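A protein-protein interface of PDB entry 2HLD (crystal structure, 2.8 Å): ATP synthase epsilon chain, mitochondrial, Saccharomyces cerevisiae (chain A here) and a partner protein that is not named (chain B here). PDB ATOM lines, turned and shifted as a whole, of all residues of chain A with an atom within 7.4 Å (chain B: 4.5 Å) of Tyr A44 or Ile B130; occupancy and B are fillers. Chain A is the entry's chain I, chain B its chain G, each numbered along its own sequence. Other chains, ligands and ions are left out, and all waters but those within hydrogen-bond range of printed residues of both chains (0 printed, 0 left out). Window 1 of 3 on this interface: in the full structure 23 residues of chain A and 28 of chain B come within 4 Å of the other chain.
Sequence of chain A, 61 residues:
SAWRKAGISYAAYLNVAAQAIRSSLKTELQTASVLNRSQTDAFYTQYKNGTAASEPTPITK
The backbone NH (N) of Ser B129 is in hydrogen-bond range of the backbone carbonyl oxygen (O) of Thr A45 (2.8 Å). N of Asn B131 is in hydrogen-bond range of O of Phe A43 (2.8 Å).
The backbone NH (N) of Thr B109 is in hydrogen-bond range of the backbone carbonyl oxygen (O) of Leu B128. The side-chain hydroxyl (OG1) of Thr B109 is in hydrogen-bond range of the side-chain hydroxyl (OG) of Ser B129 (3.3 Å). The backbone NH (N) of Ile B130 lies within hydrogen-bond range of the backbone carbonyl oxygen (O) of Thr B109 (2.7 Å). N of Gly B111 is in hydrogen-bond range of O of Ile B130, at 2.9 Å. The side-chain amide oxygen of Asn B131 sits close to the side-chain carboxylate of Asp B112 (2.7 Å). O of Ala A42 sits at hydrogen-bond distance from N of Lys A61.
CA of Ala A42 touches O of Asn B131 (3.2 Å). Ala A42 touches Ile B133. Ser B129 touches Phe A43 (O to O, 3.8 Å). O of Phe A43 touches CA of Ile B130 (3.3 Å). CD2 of Tyr A44 touches CD1 of Leu B128 (3.97 Å). Ser B129 touches Tyr A44 (O to CA, 3.3 Å). Tyr A44 touches Ile B130 (CB to CD1, 3.4 Å). CE of Lys B149 touches OH of Tyr A44 (3.7 Å). Leu B128 touches Thr A45 (CA to O, 3.6 Å). Lys A61 touches Lys B149.
Of the printed residues of chain B, Ala A42 touches Asn B131 and Ile B133. Tyr A44 touches just these residues of chain B: Leu B128, Ser B129, Ile B130 and Lys B149. Gln A46 touches none of the printed residues of chain B. Ile A59 touches none of the printed residues of chain B. Printed residues of chain A within 4 Å of Ser B129: Phe A43, Tyr A44 and Thr A45. Printed residues of chain A within 4 Å of Ile B130: Phe A43 and Tyr A44. Of the printed residues of chain A, Asn B131 touches Ala A42 (3.2 Å) and Phe A43 (2.8 Å). The nearest residue of chain A that does not touch Ile B130 is Ala A42 (4.7 Å).
Among the printed residues, 12 pairs touch across the chains.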
ATOM      1  N   ALA A  42      -8.283 -10.843  32.822  1.00  0.00           N
ATOM      2  CA  ALA A  42      -9.433 -11.695  32.575  1.00  0.00           C
ATOM      3  C   ALA A  42      -9.426 -12.350  31.188  1.00  0.00           C
ATOM      4  O   ALA A  42      -8.955 -11.760  30.219  1.00  0.00           O
ATOM      5  CB  ALA A  42     -10.708 -10.912  32.802  1.00  0.00           C
ATOM      6  N   PHE A  43      -9.951 -13.573  31.111  1.00  0.00           N
ATOM      7  CA  PHE A  43      -9.965 -14.365  29.876  1.00  0.00           C
ATOM      8  C   PHE A  43     -11.353 -14.931  29.595  1.00  0.00           C
ATOM      9  O   PHE A  43     -12.166 -15.085  30.515  1.00  0.00           O
ATOM     10  CB  PHE A  43      -8.960 -15.517  29.974  1.00  0.00           C
ATOM     11  CG  PHE A  43      -7.518 -15.076  29.955  1.00  0.00           C
ATOM     12  CD1 PHE A  43      -6.905 -14.571  31.113  1.00  0.00           C
ATOM     13  CD2 PHE A  43      -6.764 -15.174  28.785  1.00  0.00           C
ATOM     14  CE1 PHE A  43      -5.575 -14.160  31.104  1.00  0.00           C
ATOM     15  CE2 PHE A  43      -5.424 -14.764  28.760  1.00  0.00           C
ATOM     16  CZ  PHE A  43      -4.829 -14.257  29.925  1.00  0.00           C
ATOM     17  N   TYR A  44     -11.625 -15.241  28.326  1.00  0.00           N
ATOM     18  CA  TYR A  44     -12.890 -15.890  27.958  1.00  0.00           C
ATOM     19  C   TYR A  44     -12.744 -17.138  27.097  1.00  0.00           C
ATOM     20  O   TYR A  44     -12.089 -17.121  26.058  1.00  0.00           O
ATOM     21  CB  TYR A  44     -13.892 -14.894  27.355  1.00  0.00           C
ATOM     22  CG  TYR A  44     -13.568 -14.337  25.978  1.00  0.00           C
ATOM     23  CD1 TYR A  44     -12.643 -13.296  25.812  1.00  0.00           C
ATOM     24  CD2 TYR A  44     -14.226 -14.823  24.846  1.00  0.00           C
ATOM     25  CE1 TYR A  44     -12.367 -12.778  24.546  1.00  0.00           C
ATOM     26  CE2 TYR A  44     -13.958 -14.313  23.580  1.00  0.00           C
ATOM     27  CZ  TYR A  44     -13.033 -13.294  23.434  1.00  0.00           C
ATOM     28  OH  TYR A  44     -12.787 -12.799  22.173  1.00  0.00           O
ATOM     29  N   THR A  45     -13.362 -18.218  27.558  1.00  0.00           N
ATOM     30  CA  THR A  45     -13.328 -19.499  26.872  1.00  0.00           C
ATOM     31  C   THR A  45     -14.737 -19.854  26.425  1.00  0.00           C
ATOM     32  O   THR A  45     -15.692 -19.764  27.211  1.00  0.00           O
ATOM     33  CB  THR A  45     -12.786 -20.600  27.811  1.00  0.00           C
ATOM     34  OG1 THR A  45     -11.473 -20.251  28.266  1.00  0.00           O
ATOM     35  CG2 THR A  45     -12.553 -21.888  27.050  1.00  0.00           C
ATOM     36  N   GLN A  46     -14.863 -20.267  25.167  1.00  0.00           N
ATOM     37  CA  GLN A  46     -16.163 -20.645  24.612  1.00  0.00           C
ATOM     38  C   GLN A  46     -16.448 -22.127  24.853  1.00  0.00           C
ATOM     39  O   GLN A  46     -15.537 -22.948  24.822  1.00  0.00           O
ATOM     40  CB  GLN A  46     -16.218 -20.313  23.126  1.00  0.00           C
ATOM     41  CG  GLN A  46     -17.552 -19.765  22.669  1.00  0.00           C
ATOM     42  CD  GLN A  46     -17.484 -19.125  21.293  1.00  0.00           C
ATOM     43  OE1 GLN A  46     -16.431 -18.632  20.871  1.00  0.00           O
ATOM     44  NE2 GLN A  46     -18.612 -19.121  20.593  1.00  0.00           N
ATOM     45  N   TYR A  47     -17.710 -22.462  25.100  1.00  0.00           N
ATOM     46  CA  TYR A  47     -18.088 -23.825  25.479  1.00  0.00           C
ATOM     47  C   TYR A  47     -19.243 -24.392  24.642  1.00  0.00           C
ATOM     48  O   TYR A  47     -20.183 -23.666  24.299  1.00  0.00           O
ATOM     49  CB  TYR A  47     -18.460 -23.863  26.966  1.00  0.00           C
ATOM     50  CG  TYR A  47     -17.321 -24.170  27.928  1.00  0.00           C
ATOM     51  CD1 TYR A  47     -16.164 -23.381  27.969  1.00  0.00           C
ATOM     52  CD2 TYR A  47     -17.419 -25.236  28.827  1.00  0.00           C
ATOM     53  CE1 TYR A  47     -15.130 -23.660  28.865  1.00  0.00           C
ATOM     54  CE2 TYR A  47     -16.396 -25.519  29.724  1.00  0.00           C
ATOM     55  CZ  TYR A  47     -15.257 -24.729  29.737  1.00  0.00           C
ATOM     56  OH  TYR A  47     -14.250 -25.014  30.632  1.00  0.00           O
ATOM     57  N   PRO A  56     -13.765 -24.138  22.962  1.00  0.00           N
ATOM     58  CA  PRO A  56     -12.874 -23.503  21.976  1.00  0.00           C
ATOM     59  C   PRO A  56     -11.822 -22.614  22.682  1.00  0.00           C
ATOM     60  O   PRO A  56     -12.174 -21.591  23.277  1.00  0.00           O
ATOM     61  CB  PRO A  56     -13.832 -22.675  21.118  1.00  0.00           C
ATOM     62  N   THR A  57     -10.553 -23.024  22.586  1.00  0.00           N
ATOM     63  CA  THR A  57      -9.418 -22.556  23.426  1.00  0.00           C
ATOM     64  C   THR A  57      -9.371 -21.079  23.873  1.00  0.00           C
ATOM     65  O   THR A  57      -9.690 -20.170  23.099  1.00  0.00           O
ATOM     66  CB  THR A  57      -8.056 -22.962  22.776  1.00  0.00           C
ATOM     67  N   PRO A  58      -8.925 -20.880  25.122  1.00  0.00           N
ATOM     68  CA  PRO A  58      -8.980 -19.598  25.849  1.00  0.00           C
ATOM     69  C   PRO A  58      -8.403 -18.390  25.104  1.00  0.00           C
ATOM     70  O   PRO A  58      -7.433 -18.535  24.359  1.00  0.00           O
ATOM     71  CB  PRO A  58      -8.151 -19.886  27.104  1.00  0.00           C
ATOM     72  N   ILE A  59      -9.001 -17.216  25.307  1.00  0.00           N
ATOM     73  CA  ILE A  59      -8.559 -15.975  24.664  1.00  0.00           C
ATOM     74  C   ILE A  59      -8.616 -14.813  25.651  1.00  0.00           C
ATOM     75  O   ILE A  59      -9.486 -14.780  26.519  1.00  0.00           O
ATOM     76  CB  ILE A  59      -9.430 -15.666  23.428  1.00  0.00           C
ATOM     77  N   THR A  60      -7.696 -13.861  25.525  1.00  0.00           N
ATOM     78  CA  THR A  60      -7.685 -12.700  26.423  1.00  0.00           C
ATOM     79  C   THR A  60      -8.907 -11.794  26.195  1.00  0.00           C
ATOM     80  O   THR A  60      -9.312 -11.567  25.057  1.00  0.00           O
ATOM     81  CB  THR A  60      -6.366 -11.903  26.279  1.00  0.00           C
ATOM     82  N   LYS A  61      -9.496 -11.297  27.282  1.00  0.00           N
ATOM     83  CA  LYS A  61     -10.650 -10.401  27.206  1.00  0.00           C
ATOM     84  C   LYS A  61     -10.300  -9.095  26.493  1.00  0.00           C
ATOM     85  O   LYS A  61     -11.160  -8.239  26.297  1.00  0.00           O
ATOM     86  CB  LYS A  61     -11.227 -10.122  28.605  1.00  0.00           C
ATOM     87  N   THR B 109     -20.904 -18.154  32.516  1.00  0.00           N
ATOM     88  CA  THR B 109     -20.300 -18.196  33.851  1.00  0.00           C
ATOM     89  C   THR B 109     -19.175 -17.180  33.986  1.00  0.00           C
ATOM     90  O   THR B 109     -18.255 -17.113  33.155  1.00  0.00           O
ATOM     91  CB  THR B 109     -19.783 -19.632  34.219  1.00  0.00           C
ATOM     92  OG1 THR B 109     -18.923 -20.144  33.179  1.00  0.00           O
ATOM     93  CG2 THR B 109     -20.934 -20.613  34.258  1.00  0.00           C
ATOM     94  N   ILE B 110     -19.250 -16.386  35.039  1.00  0.00           N
ATOM     95  CA  ILE B 110     -18.151 -15.499  35.342  1.00  0.00           C
ATOM     96  C   ILE B 110     -17.509 -16.024  36.602  1.00  0.00           C
ATOM     97  O   ILE B 110     -18.096 -15.954  37.689  1.00  0.00           O
ATOM     98  CB  ILE B 110     -18.620 -14.017  35.424  1.00  0.00           C
ATOM     99  CG1 ILE B 110     -19.102 -13.573  34.033  1.00  0.00           C
ATOM    100  CG2 ILE B 110     -17.491 -13.101  35.926  1.00  0.00           C
ATOM    101  CD1 ILE B 110     -19.748 -12.175  33.982  1.00  0.00           C
ATOM    102  N   GLY B 111     -16.317 -16.596  36.423  1.00  0.00           N
ATOM    103  CA  GLY B 111     -15.562 -17.229  37.521  1.00  0.00           C
ATOM    104  C   GLY B 111     -15.569 -18.751  37.482  1.00  0.00           C
ATOM    105  O   GLY B 111     -16.630 -19.350  37.382  1.00  0.00           O
ATOM    106  N   ASP B 112     -14.392 -19.375  37.577  1.00  0.00           N
ATOM    107  CA  ASP B 112     -14.247 -20.839  37.443  1.00  0.00           C
ATOM    108  C   ASP B 112     -15.056 -21.712  38.395  1.00  0.00           C
ATOM    109  O   ASP B 112     -15.531 -22.769  37.988  1.00  0.00           O
ATOM    110  CB  ASP B 112     -12.793 -21.243  37.579  1.00  0.00           C
ATOM    111  CG  ASP B 112     -12.044 -21.150  36.279  1.00  0.00           C
ATOM    112  OD1 ASP B 112     -12.675 -21.283  35.205  1.00  0.00           O
ATOM    113  OD2 ASP B 112     -10.811 -20.957  36.235  1.00  0.00           O
ATOM    114  N   LEU B 128     -20.309 -19.787  27.353  1.00  0.00           N
ATOM    115  CA  LEU B 128     -19.196 -18.862  27.541  1.00  0.00           C
ATOM    116  C   LEU B 128     -18.744 -18.876  28.995  1.00  0.00           C
ATOM    117  O   LEU B 128     -19.570 -18.898  29.917  1.00  0.00           O
ATOM    118  CB  LEU B 128     -19.587 -17.436  27.109  1.00  0.00           C
ATOM    119  CG  LEU B 128     -18.492 -16.381  26.944  1.00  0.00           C
ATOM    120  CD1 LEU B 128     -17.542 -16.768  25.833  1.00  0.00           C
ATOM    121  CD2 LEU B 128     -19.111 -15.032  26.661  1.00  0.00           C
ATOM    122  N   SER B 129     -17.429 -18.882  29.195  1.00  0.00           N
ATOM    123  CA  SER B 129     -16.881 -18.809  30.535  1.00  0.00           C
ATOM    124  C   SER B 129     -15.811 -17.746  30.659  1.00  0.00           C
ATOM    125  O   SER B 129     -14.840 -17.751  29.909  1.00  0.00           O
ATOM    126  CB  SER B 129     -16.308 -20.143  30.973  1.00  0.00           C
ATOM    127  OG  SER B 129     -15.772 -20.008  32.280  1.00  0.00           O
ATOM    128  N   ILE B 130     -16.011 -16.849  31.620  1.00  0.00           N
ATOM    129  CA  ILE B 130     -15.068 -15.784  31.916  1.00  0.00           C
ATOM    130  C   ILE B 130     -14.228 -16.185  33.112  1.00  0.00           C
ATOM    131  O   ILE B 130     -14.713 -16.828  34.058  1.00  0.00           O
ATOM    132  CB  ILE B 130     -15.797 -14.447  32.204  1.00  0.00           C
ATOM    133  CG1 ILE B 130     -16.811 -14.133  31.101  1.00  0.00           C
ATOM    134  CG2 ILE B 130     -14.789 -13.303  32.435  1.00  0.00           C
ATOM    135  CD1 ILE B 130     -16.244 -14.124  29.712  1.00  0.00           C
ATOM    136  N   ASN B 131     -12.982 -15.732  33.085  1.00  0.00           N
ATOM    137  CA  ASN B 131     -11.923 -16.341  33.850  1.00  0.00           C
ATOM    138  C   ASN B 131     -10.993 -15.349  34.516  1.00  0.00           C
ATOM    139  O   ASN B 131     -10.763 -14.272  33.986  1.00  0.00           O
ATOM    140  CB  ASN B 131     -11.108 -17.183  32.890  1.00  0.00           C
ATOM    141  CG  ASN B 131     -10.455 -18.305  33.561  1.00  0.00           C
ATOM    142  OD1 ASN B 131     -11.076 -19.009  34.341  1.00  0.00           O
ATOM    143  ND2 ASN B 131      -9.184 -18.493  33.280  1.00  0.00           N
ATOM    144  N   ILE B 133     -10.981 -13.706  37.737  1.00  0.00           N
ATOM    145  CA  ILE B 133     -11.686 -12.553  38.270  1.00  0.00           C
ATOM    146  C   ILE B 133     -11.389 -12.392  39.753  1.00  0.00           C
ATOM    147  O   ILE B 133     -11.358 -11.269  40.275  1.00  0.00           O
ATOM    148  CB  ILE B 133     -13.216 -12.712  38.018  1.00  0.00           C
ATOM    149  CG1 ILE B 133     -13.530 -12.590  36.519  1.00  0.00           C
ATOM    150  CG2 ILE B 133     -14.039 -11.692  38.832  1.00  0.00           C
ATOM    151  CD1 ILE B 133     -13.025 -11.293  35.853  1.00  0.00           C
ATOM    152  N   ILE B 146     -16.586  -7.662  29.149  1.00  0.00           N
ATOM    153  CA  ILE B 146     -17.458  -8.822  29.283  1.00  0.00           C
ATOM    154  C   ILE B 146     -18.768  -8.552  28.550  1.00  0.00           C
ATOM    155  O   ILE B 146     -19.200  -9.369  27.711  1.00  0.00           O
ATOM    156  CB  ILE B 146     -17.726  -9.155  30.762  1.00  0.00           C
ATOM    157  CG1 ILE B 146     -16.462  -9.705  31.435  1.00  0.00           C
ATOM    158  CG2 ILE B 146     -18.871 -10.167  30.878  1.00  0.00           C
ATOM    159  CD1 ILE B 146     -16.548  -9.768  32.960  1.00  0.00           C
ATOM    160  N   LYS B 149     -18.664  -9.078  24.880  1.00  0.00           N
ATOM    161  CA  LYS B 149     -18.640 -10.391  24.287  1.00  0.00           C
ATOM    162  C   LYS B 149     -20.039 -10.982  24.313  1.00  0.00           C
ATOM    163  O   LYS B 149     -20.456 -11.681  23.387  1.00  0.00           O
ATOM    164  CB  LYS B 149     -17.638 -11.266  25.027  1.00  0.00           C
ATOM    165  CG  LYS B 149     -16.223 -10.708  25.014  1.00  0.00           C
ATOM    166  CD  LYS B 149     -15.727 -10.468  23.588  1.00  0.00           C
ATOM    167  CE  LYS B 149     -14.358  -9.799  23.572  1.00  0.00           C
ATOM    168  NZ  LYS B 149     -14.323  -8.530  24.369  1.00  0.00           N
